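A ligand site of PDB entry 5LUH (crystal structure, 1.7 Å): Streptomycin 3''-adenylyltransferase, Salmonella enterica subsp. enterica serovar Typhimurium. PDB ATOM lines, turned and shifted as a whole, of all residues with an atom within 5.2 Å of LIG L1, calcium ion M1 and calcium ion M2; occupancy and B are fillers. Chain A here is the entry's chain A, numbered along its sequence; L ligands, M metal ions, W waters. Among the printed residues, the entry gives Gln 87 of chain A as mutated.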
ATOM      1  N   GLY A  35       6.525  21.761 -15.193  1.00  0.00           N
ATOM      2  CA  GLY A  35       5.779  20.495 -15.150  1.00  0.00           C
ATOM      3  C   GLY A  35       4.439  20.592 -15.856  1.00  0.00           C
ATOM      4  O   GLY A  35       4.196  21.519 -16.628  1.00  0.00           O
ATOM      5  N   SER A  36       3.530  19.646 -15.558  1.00  0.00           N
ATOM      6  CA  SER A  36       2.355  19.486 -16.406  1.00  0.00           C
ATOM      7  C   SER A  36       1.376  20.669 -16.288  1.00  0.00           C
ATOM      8  O   SER A  36       0.597  20.896 -17.217  1.00  0.00           O
ATOM      9  CB  SER A  36       1.643  18.164 -16.090  1.00  0.00           C
ATOM     10  OG  SER A  36       1.088  18.153 -14.770  1.00  0.00           O
ATOM     11  N   ASP A  47       0.310  16.921  -9.354  1.00  0.00           N
ATOM     12  CA  ASP A  47       0.818  17.896  -8.393  1.00  0.00           C
ATOM     13  C   ASP A  47       1.113  19.231  -9.099  1.00  0.00           C
ATOM     14  O   ASP A  47       1.010  19.365 -10.318  1.00  0.00           O
ATOM     15  CB  ASP A  47       2.050  17.360  -7.674  1.00  0.00           C
ATOM     16  CG  ASP A  47       3.132  16.851  -8.615  1.00  0.00           C
ATOM     17  OD1 ASP A  47       2.982  16.965  -9.839  1.00  0.00           O
ATOM     18  OD2 ASP A  47       4.165  16.359  -8.110  1.00  0.00           O
ATOM     19  N   ASP A  49       4.214  21.684  -9.654  1.00  0.00           N
ATOM     20  CA  ASP A  49       5.682  21.554  -9.573  1.00  0.00           C
ATOM     21  C   ASP A  49       6.325  22.943  -9.451  1.00  0.00           C
ATOM     22  O   ASP A  49       6.139  23.796 -10.327  1.00  0.00           O
ATOM     23  CB  ASP A  49       6.226  20.841 -10.813  1.00  0.00           C
ATOM     24  CG  ASP A  49       5.687  19.437 -10.980  1.00  0.00           C
ATOM     25  OD1 ASP A  49       5.498  18.719  -9.983  1.00  0.00           O
ATOM     26  OD2 ASP A  49       5.459  19.039 -12.139  1.00  0.00           O
ATOM     27  N   GLN A  87       4.816  19.931  -5.057  1.00  0.00           N
ATOM     28  CA  GLN A  87       6.188  19.459  -5.080  1.00  0.00           C
ATOM     29  C   GLN A  87       7.091  20.683  -5.147  1.00  0.00           C
ATOM     30  O   GLN A  87       6.978  21.491  -6.083  1.00  0.00           O
ATOM     31  CB  GLN A  87       6.469  18.520  -6.254  1.00  0.00           C
ATOM     32  CG  GLN A  87       7.916  18.016  -6.244  1.00  0.00           C
ATOM     33  CD  GLN A  87       8.213  16.988  -7.317  1.00  0.00           C
ATOM     34  OE1 GLN A  87       7.643  15.904  -7.339  1.00  0.00           O
ATOM     35  NE2 GLN A  87       9.141  17.320  -8.199  1.00  0.00           N
ATOM     36  N   GLN A 108      13.684  18.924  -0.681  1.00  0.00           N
ATOM     37  CA  GLN A 108      12.555  18.546  -1.521  1.00  0.00           C
ATOM     38  C   GLN A 108      11.357  18.294  -0.617  1.00  0.00           C
ATOM     39  O   GLN A 108      11.442  17.523   0.341  1.00  0.00           O
ATOM     40  CB  GLN A 108      12.854  17.309  -2.375  1.00  0.00           C
ATOM     41  CG  GLN A 108      11.908  17.180  -3.568  1.00  0.00           C
ATOM     42  CD  GLN A 108      12.393  16.186  -4.614  1.00  0.00           C
ATOM     43  OE1 GLN A 108      12.618  15.016  -4.314  1.00  0.00           O
ATOM     44  NE2 GLN A 108      12.548  16.660  -5.850  1.00  0.00           N
ATOM     45  N   TRP A 112       4.687  12.328  -1.000  1.00  0.00           N
ATOM     46  CA  TRP A 112       5.219  11.008  -0.693  1.00  0.00           C
ATOM     47  C   TRP A 112       6.080  11.012   0.567  1.00  0.00           C
ATOM     48  O   TRP A 112       6.406   9.933   1.077  1.00  0.00           O
ATOM     49  CB  TRP A 112       5.995  10.462  -1.913  1.00  0.00           C
ATOM     50  CG  TRP A 112       7.354  11.118  -2.194  1.00  0.00           C
ATOM     51  CD1 TRP A 112       8.573  10.693  -1.749  1.00  0.00           C
ATOM     52  CD2 TRP A 112       7.602  12.303  -2.969  1.00  0.00           C
ATOM     53  NE1 TRP A 112       9.566  11.541  -2.193  1.00  0.00           N
ATOM     54  CE2 TRP A 112       8.998  12.531  -2.941  1.00  0.00           C
ATOM     55  CE3 TRP A 112       6.779  13.175  -3.683  1.00  0.00           C
ATOM     56  CZ2 TRP A 112       9.587  13.610  -3.603  1.00  0.00           C
ATOM     57  CZ3 TRP A 112       7.368  14.244  -4.341  1.00  0.00           C
ATOM     58  CH2 TRP A 112       8.759  14.455  -4.300  1.00  0.00           C
ATOM     59  N   ASP A 130      18.449  14.029 -11.507  1.00  0.00           N
ATOM     60  CA  ASP A 130      17.237  14.553 -12.122  1.00  0.00           C
ATOM     61  C   ASP A 130      17.223  16.077 -12.184  1.00  0.00           C
ATOM     62  O   ASP A 130      16.537  16.633 -13.043  1.00  0.00           O
ATOM     63  CB  ASP A 130      15.998  14.031 -11.381  1.00  0.00           C
ATOM     64  CG  ASP A 130      14.699  14.351 -12.134  1.00  0.00           C
ATOM     65  OD1 ASP A 130      14.547  13.871 -13.279  1.00  0.00           O
ATOM     66  OD2 ASP A 130      13.863  15.088 -11.593  1.00  0.00           O
ATOM     67  N   PRO A 169      18.410   6.815 -14.335  1.00  0.00           N
ATOM     68  CA  PRO A 169      17.388   5.931 -13.746  1.00  0.00           C
ATOM     69  C   PRO A 169      17.196   4.660 -14.548  1.00  0.00           C
ATOM     70  O   PRO A 169      16.818   3.634 -13.993  1.00  0.00           O
ATOM     71  CB  PRO A 169      16.122   6.802 -13.729  1.00  0.00           C
ATOM     72  CG  PRO A 169      16.325   7.790 -14.815  1.00  0.00           C
ATOM     73  CD  PRO A 169      17.817   8.032 -14.927  1.00  0.00           C
ATOM     74  N   LEU A 172      19.348   2.035 -13.210  1.00  0.00           N
ATOM     75  CA  LEU A 172      19.011   1.690 -11.825  1.00  0.00           C
ATOM     76  C   LEU A 172      17.764   0.805 -11.708  1.00  0.00           C
ATOM     77  O   LEU A 172      17.653   0.046 -10.734  1.00  0.00           O
ATOM     78  CB  LEU A 172      18.815   2.963 -10.997  1.00  0.00           C
ATOM     79  CG  LEU A 172      18.478   2.841  -9.505  1.00  0.00           C
ATOM     80  CD1 LEU A 172      19.184   3.921  -8.707  1.00  0.00           C
ATOM     81  CD2 LEU A 172      16.952   2.886  -9.243  1.00  0.00           C
ATOM     82  N   TRP A 173      16.818   0.903 -12.636  1.00  0.00           N
ATOM     83  CA  TRP A 173      15.660   0.010 -12.598  1.00  0.00           C
ATOM     84  C   TRP A 173      16.082  -1.384 -13.052  1.00  0.00           C
ATOM     85  O   TRP A 173      16.419  -1.583 -14.225  1.00  0.00           O
ATOM     86  CB  TRP A 173      14.538   0.521 -13.480  1.00  0.00           C
ATOM     87  CG  TRP A 173      13.829   1.717 -12.965  1.00  0.00           C
ATOM     88  CD1 TRP A 173      13.334   1.894 -11.708  1.00  0.00           C
ATOM     89  CD2 TRP A 173      13.499   2.882 -13.702  1.00  0.00           C
ATOM     90  NE1 TRP A 173      12.742   3.132 -11.612  1.00  0.00           N
ATOM     91  CE2 TRP A 173      12.823   3.763 -12.829  1.00  0.00           C
ATOM     92  CE3 TRP A 173      13.717   3.289 -15.022  1.00  0.00           C
ATOM     93  CZ2 TRP A 173      12.369   5.006 -13.229  1.00  0.00           C
ATOM     94  CZ3 TRP A 173      13.264   4.532 -15.422  1.00  0.00           C
ATOM     95  CH2 TRP A 173      12.586   5.368 -14.525  1.00  0.00           C
ATOM     96  N   ALA A 177      11.656  -5.435  -7.089  1.00  0.00           N
ATOM     97  CA  ALA A 177      11.484  -4.488  -5.990  1.00  0.00           C
ATOM     98  C   ALA A 177      11.847  -3.059  -6.384  1.00  0.00           C
ATOM     99  O   ALA A 177      11.336  -2.122  -5.765  1.00  0.00           O
ATOM    100  CB  ALA A 177      12.339  -4.914  -4.786  1.00  0.00           C
ATOM    101  N   ASP A 178      12.708  -2.870  -7.393  1.00  0.00           N
ATOM    102  CA  ASP A 178      13.015  -1.527  -7.881  1.00  0.00           C
ATOM    103  C   ASP A 178      11.769  -0.839  -8.446  1.00  0.00           C
ATOM    104  O   ASP A 178      11.680   0.399  -8.411  1.00  0.00           O
ATOM    105  CB  ASP A 178      14.099  -1.574  -8.967  1.00  0.00           C
ATOM    106  CG  ASP A 178      15.457  -1.996  -8.420  1.00  0.00           C
ATOM    107  OD1 ASP A 178      15.716  -1.826  -7.221  1.00  0.00           O
ATOM    108  OD2 ASP A 178      16.267  -2.493  -9.232  1.00  0.00           O
ATOM    109  N   VAL A 179      10.821  -1.602  -8.972  1.00  0.00           N
ATOM    110  CA  VAL A 179       9.672  -1.049  -9.675  1.00  0.00           C
ATOM    111  C   VAL A 179       8.361  -1.227  -8.907  1.00  0.00           C
ATOM    112  O   VAL A 179       7.392  -0.496  -9.198  1.00  0.00           O
ATOM    113  CB  VAL A 179       9.531  -1.632 -11.100  1.00  0.00           C
ATOM    114  CG1 VAL A 179      10.795  -1.365 -11.928  1.00  0.00           C
ATOM    115  CG2 VAL A 179       9.210  -3.115 -11.038  1.00  0.00           C
ATOM    116  N   GLN A 180       8.291  -2.161  -7.956  1.00  0.00           N
ATOM    117  CA  GLN A 180       7.055  -2.407  -7.224  1.00  0.00           C
ATOM    118  C   GLN A 180       6.578  -1.134  -6.527  1.00  0.00           C
ATOM    119  O   GLN A 180       7.377  -0.385  -5.957  1.00  0.00           O
ATOM    120  CB  GLN A 180       7.282  -3.530  -6.194  1.00  0.00           C
ATOM    121  CG  GLN A 180       6.015  -4.120  -5.566  1.00  0.00           C
ATOM    122  CD  GLN A 180       5.438  -3.237  -4.466  1.00  0.00           C
ATOM    123  OE1 GLN A 180       6.174  -2.599  -3.710  1.00  0.00           O
ATOM    124  NE2 GLN A 180       4.112  -3.196  -4.374  1.00  0.00           N
ATOM    125  N   ASP A 182       5.457   1.497  -8.100  1.00  0.00           N
ATOM    126  CA  ASP A 182       5.534   2.621  -9.035  1.00  0.00           C
ATOM    127  C   ASP A 182       5.402   2.132 -10.470  1.00  0.00           C
ATOM    128  O   ASP A 182       5.979   2.717 -11.384  1.00  0.00           O
ATOM    129  CB  ASP A 182       6.845   3.400  -8.882  1.00  0.00           C
ATOM    130  CG  ASP A 182       6.881   4.251  -7.624  1.00  0.00           C
ATOM    131  OD1 ASP A 182       6.217   5.310  -7.606  1.00  0.00           O
ATOM    132  OD2 ASP A 182       7.589   3.864  -6.666  1.00  0.00           O
ATOM    133  N   HIS A 185       3.976   4.514 -13.263  1.00  0.00           N
ATOM    134  CA  HIS A 185       4.853   5.674 -13.347  1.00  0.00           C
ATOM    135  C   HIS A 185       6.142   5.311 -14.088  1.00  0.00           C
ATOM    136  O   HIS A 185       6.613   6.074 -14.948  1.00  0.00           O
ATOM    137  CB  HIS A 185       5.173   6.207 -11.948  1.00  0.00           C
ATOM    138  CG  HIS A 185       6.045   7.437 -11.960  1.00  0.00           C
ATOM    139  ND1 HIS A 185       5.630   8.641 -12.478  1.00  0.00           N
ATOM    140  CD2 HIS A 185       7.316   7.634 -11.539  1.00  0.00           C
ATOM    141  CE1 HIS A 185       6.598   9.527 -12.379  1.00  0.00           C
ATOM    142  NE2 HIS A 185       7.635   8.944 -11.803  1.00  0.00           N
ATOM    143  N   ILE A 186       6.714   4.160 -13.771  1.00  0.00           N
ATOM    144  CA  ILE A 186       8.009   3.814 -14.352  1.00  0.00           C
ATOM    145  C   ILE A 186       7.854   3.488 -15.833  1.00  0.00           C
ATOM    146  O   ILE A 186       8.682   3.901 -16.662  1.00  0.00           O
ATOM    147  CB  ILE A 186       8.632   2.637 -13.577  1.00  0.00           C
ATOM    148  CG1 ILE A 186       9.095   3.135 -12.206  1.00  0.00           C
ATOM    149  CG2 ILE A 186       9.812   2.052 -14.353  1.00  0.00           C
ATOM    150  CD1 ILE A 186       9.494   2.040 -11.306  1.00  0.00           C
ATOM    151  N   THR A 189       7.485   6.784 -17.563  1.00  0.00           N
ATOM    152  CA  THR A 189       8.722   7.562 -17.560  1.00  0.00           C
ATOM    153  C   THR A 189       9.731   6.975 -18.539  1.00  0.00           C
ATOM    154  O   THR A 189      10.405   7.726 -19.248  1.00  0.00           O
ATOM    155  CB  THR A 189       9.291   7.619 -16.141  1.00  0.00           C
ATOM    156  OG1 THR A 189       8.335   8.269 -15.299  1.00  0.00           O
ATOM    157  CG2 THR A 189      10.617   8.414 -16.097  1.00  0.00           C
HETATM  158  C1  LIG L   1      11.864   3.892  -6.556  1.00  0.00           C
HETATM  159  N1  LIG L   1      11.591   2.552  -6.043  1.00  0.00           N
HETATM  160  C2  LIG L   1      12.459   1.804  -5.476  1.00  0.00           C
HETATM  161  N2  LIG L   1      13.680   2.331  -5.390  1.00  0.00           N
HETATM  162  N3  LIG L   1      12.271   0.576  -4.981  1.00  0.00           N
HETATM  163  C3  LIG L   1      11.110   4.928  -5.731  1.00  0.00           C
HETATM  164  O1  LIG L   1      11.534   4.865  -4.379  1.00  0.00           O
HETATM  165  C4  LIG L   1      11.289   6.335  -6.291  1.00  0.00           C
HETATM  166  N4  LIG L   1      10.515   7.270  -5.499  1.00  0.00           N
HETATM  167  C5  LIG L   1      11.026   8.112  -4.693  1.00  0.00           C
HETATM  168  N5  LIG L   1      10.141   8.867  -4.057  1.00  0.00           N
HETATM  169  N6  LIG L   1      12.325   8.313  -4.445  1.00  0.00           N
HETATM  170  C6  LIG L   1      10.836   6.375  -7.750  1.00  0.00           C
HETATM  171  O2  LIG L   1      11.193   7.673  -8.232  1.00  0.00           O
HETATM  172  C7  LIG L   1      11.569   5.343  -8.586  1.00  0.00           C
HETATM  173  O3  LIG L   1      11.122   5.369  -9.941  1.00  0.00           O
HETATM  174  C8  LIG L   1      11.365   3.955  -7.997  1.00  0.00           C
HETATM  175  O4  LIG L   1      12.044   2.987  -8.785  1.00  0.00           O
HETATM  176  C9  LIG L   1      10.266   8.350  -9.058  1.00  0.00           C
HETATM  177  C10 LIG L   1      10.577   9.848  -8.900  1.00  0.00           C
HETATM  178  C11 LIG L   1      10.966  10.284 -10.320  1.00  0.00           C
HETATM  179  O5  LIG L   1       9.807  10.720 -11.073  1.00  0.00           O
HETATM  180  C12 LIG L   1      11.959  11.433 -10.390  1.00  0.00           C
HETATM  181  O6  LIG L   1      13.095  11.254 -10.034  1.00  0.00           O
HETATM  182  C13 LIG L   1      11.544   8.976 -10.890  1.00  0.00           C
HETATM  183  C14 LIG L   1      11.611   8.896 -12.394  1.00  0.00           C
HETATM  184  O7  LIG L   1      10.641   7.975 -10.368  1.00  0.00           O
HETATM  185  O8  LIG L   1       9.423  10.596  -8.504  1.00  0.00           O
HETATM  186  C15 LIG L   1       9.322  10.890  -7.133  1.00  0.00           C
HETATM  187  C16 LIG L   1       8.565  12.202  -6.951  1.00  0.00           C
HETATM  188  N7  LIG L   1       9.253  13.295  -7.639  1.00  0.00           N
HETATM  189  C17 LIG L   1      10.653  13.446  -7.243  1.00  0.00           C
HETATM  190  C18 LIG L   1       7.137  12.019  -7.451  1.00  0.00           C
HETATM  191  O9  LIG L   1       6.381  13.213  -7.212  1.00  0.00           O
HETATM  192  C19 LIG L   1       6.489  10.847  -6.731  1.00  0.00           C
HETATM  193  O10 LIG L   1       5.172  10.631  -7.217  1.00  0.00           O
HETATM  194  C20 LIG L   1       7.323   9.589  -6.911  1.00  0.00           C
HETATM  195  O11 LIG L   1       8.673   9.831  -6.454  1.00  0.00           O
HETATM  196  C21 LIG L   1       6.794   8.414  -6.126  1.00  0.00           C
HETATM  197  O12 LIG L   1       7.699   7.321  -6.148  1.00  0.00           O
HETATM  198  P1  LG2 L   2       1.976  14.873 -13.588  1.00  0.00           P
HETATM  199  O1  LG2 L   2       1.660  13.421 -13.416  1.00  0.00           O
HETATM  200  O2  LG2 L   2       2.568  15.443 -12.329  1.00  0.00           O
HETATM  201  O3  LG2 L   2       0.756  15.698 -14.056  1.00  0.00           O
HETATM  202  P2  LG2 L   2       4.479  15.672 -14.844  1.00  0.00           P
HETATM  203  O4  LG2 L   2       4.929  15.752 -16.288  1.00  0.00           O
HETATM  204  O5  LG2 L   2       4.469  16.984 -14.149  1.00  0.00           O
HETATM  205  O6  LG2 L   2       3.042  14.970 -14.772  1.00  0.00           O
HETATM  206  P3  LG2 L   2       6.165  14.600 -12.667  1.00  0.00           P
HETATM  207  O7  LG2 L   2       5.926  13.209 -12.103  1.00  0.00           O
HETATM  208  O8  LG2 L   2       5.778  15.694 -11.762  1.00  0.00           O
HETATM  209  O9  LG2 L   2       5.416  14.653 -14.074  1.00  0.00           O
HETATM  210  O10 LG2 L   2       7.678  14.738 -13.124  1.00  0.00           O
HETATM  211  C1  LG2 L   2       8.229  13.733 -13.994  1.00  0.00           C
HETATM  212  C2  LG2 L   2       9.583  13.339 -13.458  1.00  0.00           C
HETATM  213  O11 LG2 L   2      10.211  12.411 -14.379  1.00  0.00           O
HETATM  214  C3  LG2 L   2      10.545  14.494 -13.299  1.00  0.00           C
HETATM  215  O12 LG2 L   2      11.409  14.270 -12.189  1.00  0.00           O
HETATM  216  C4  LG2 L   2      11.307  14.464 -14.630  1.00  0.00           C
HETATM  217  O13 LG2 L   2      12.561  15.117 -14.595  1.00  0.00           O
HETATM  218  C5  LG2 L   2      11.441  12.954 -14.804  1.00  0.00           C
HETATM  219  N1  LG2 L   2      11.750  12.509 -16.163  1.00  0.00           N
HETATM  220  C6  LG2 L   2      12.731  11.606 -16.480  1.00  0.00           C
HETATM  221  N2  LG2 L   2      12.970  11.515 -17.761  1.00  0.00           N
HETATM  222  C7  LG2 L   2      12.075  12.400 -18.328  1.00  0.00           C
HETATM  223  C8  LG2 L   2      11.839  12.784 -19.665  1.00  0.00           C
HETATM  224  N3  LG2 L   2      12.514  12.297 -20.718  1.00  0.00           N
HETATM  225  N4  LG2 L   2      10.864  13.693 -19.907  1.00  0.00           N
HETATM  226  C9  LG2 L   2      10.174  14.178 -18.854  1.00  0.00           C
HETATM  227  N5  LG2 L   2      10.317  13.906 -17.559  1.00  0.00           N
HETATM  228  C10 LG2 L   2      11.299  13.004 -17.356  1.00  0.00           C
HETATM  229 CA    CA M   1       6.386  16.323  -9.429  1.00  0.00          CA
HETATM  230 CA    CA M   2       3.991  17.212 -11.815  1.00  0.00          CA
HETATM  231  O   HOH W   1       2.203  18.601 -12.470  1.00  0.00           O
HETATM  232  O   HOH W   2       5.261  14.066  -9.311  1.00  0.00           O
HETATM  233  O   HOH W   3      15.086   9.977 -11.627  1.00  0.00           O
HETATM  234  O   HOH W   4       9.062   1.580  -6.508  1.00  0.00           O
HETATM  235  O   HOH W   5       8.839  17.358 -11.016  1.00  0.00           O
HETATM  236  O   HOH W   6       8.370  13.082 -10.373  1.00  0.00           O
HETATM  237  O   HOH W   7      14.166  13.100  -7.836  1.00  0.00           O
HETATM  238  O   HOH W   8      12.220  10.296  -1.919  1.00  0.00           O
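An oxygen (O9) of LIG L1 lies close to the side-chain amide oxygen (OE1) of Gln 87 (3.0 Å).
O of Asp 178 lies within hydrogen-bond range of O4 of LIG L1, at 2.6 Å.
The side-chain carboxylate (OD1) of Asp 182 is in hydrogen-bond range of an oxygen (O12) of LIG L1 (2.9 Å).
A ring nitrogen (NE2) of His 185 sits at hydrogen-bond distance from an oxygen (O5) of LIG L1, 2.9 Å away.
An oxygen (O4) of LIG L1 lies within hydrogen-bond range of the indole nitrogen (NE1) of Trp 173 (2.9 Å).
The backbone carbonyl oxygen (O) of Ala 177 lies within hydrogen-bond range of a nitrogen (N3) of LIG L1 (3.0 Å).
The side-chain carboxylate (OD2) of Asp 130 is in hydrogen-bond range of an oxygen (O12) of LG2 L2, at 2.7 Å.
N of Ser 36 lies close to O5 of LG2 L2, at 3.2 Å.
The side-chain hydroxyl (OG) of Ser 36 sits at hydrogen-bond distance from an oxygen (O3) of LG2 L2, 2.6 Å away.
OG1 of Thr 189 sits at hydrogen-bond distance from O of His 185, 2.8 Å away.
The indole nitrogen (NE1) of Trp 112 lies close to a nitrogen (N5) of LIG L1 (3.3 Å).
Gln 108 touches LIG L1.
Ile 186 touches LIG L1.
CG2 of Thr 189 touches C14 of LIG L1 (3.9 Å).
Hydrophobic or aromatic side chains that line LIG L1: Trp 112, Trp 173, His 185 and Ile 186.
11 residues have an atom within 4 Å of LIG L1: Asp 47, Gln 87, Gln 108, Trp 112, Trp 173, Ala 177, Asp 178, Asp 182, His 185, Ile 186 and Thr 189.
Within 4 Å of calcium ion M1: Asp 47, Asp 49 and Gln 87.
Along chain A the residues within 4 Å of calcium ion M1 span positions 47 to 87.
The nearest printed residue that does not touch calcium ion M1 is Trp 112 (5.6 Å).
Within 4 Å of calcium ion M2: Asp 47 and Asp 49.
Calcium ion M1 is bound by OE1 of Gln 87 (2.5 Å), O8 of LG2 L2 (2.5 Å), water W2 (2.5 Å), OD2 of Asp 47 (2.6 Å) and OD1 of Asp 49 (2.6 Å).
Slightly farther from calcium ion M1 lies water W5 (3.1 Å).
Calcium ion M2 is bound by the side-chain carboxylate (OD1) of Asp 47 (2.2 Å), an oxygen (O2) of LG2 L2 (2.3 Å), an oxygen (O8) of LG2 L2 (2.3 Å), water W1 (2.4 Å), the side-chain carboxylate (OD2) of Asp 49 (2.4 Å), an oxygen (O5) of LG2 L2 (2.4 Å) and the side-chain carboxylate (OD1) of Asp 49 (2.8 Å).
Calcium ion M2 has seven donor atoms within binding distance.
Water W2 lies within hydrogen-bond range of an oxygen (O9) of LIG L1 (2.5 Å) and an oxygen (O7) of LG2 L2 (3.0 Å).
Water W1 bridges O of Asp 47 (2.6 Å) and OG of Ser 36 (2.6 Å).
Water W6 lies within hydrogen-bond range of O5 of LIG L1 (2.9 Å) and O7 of LG2 L2 (3.0 Å).
Water W8 lies within hydrogen-bond range of NE1 of Trp 112 and N6 of LIG L1.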
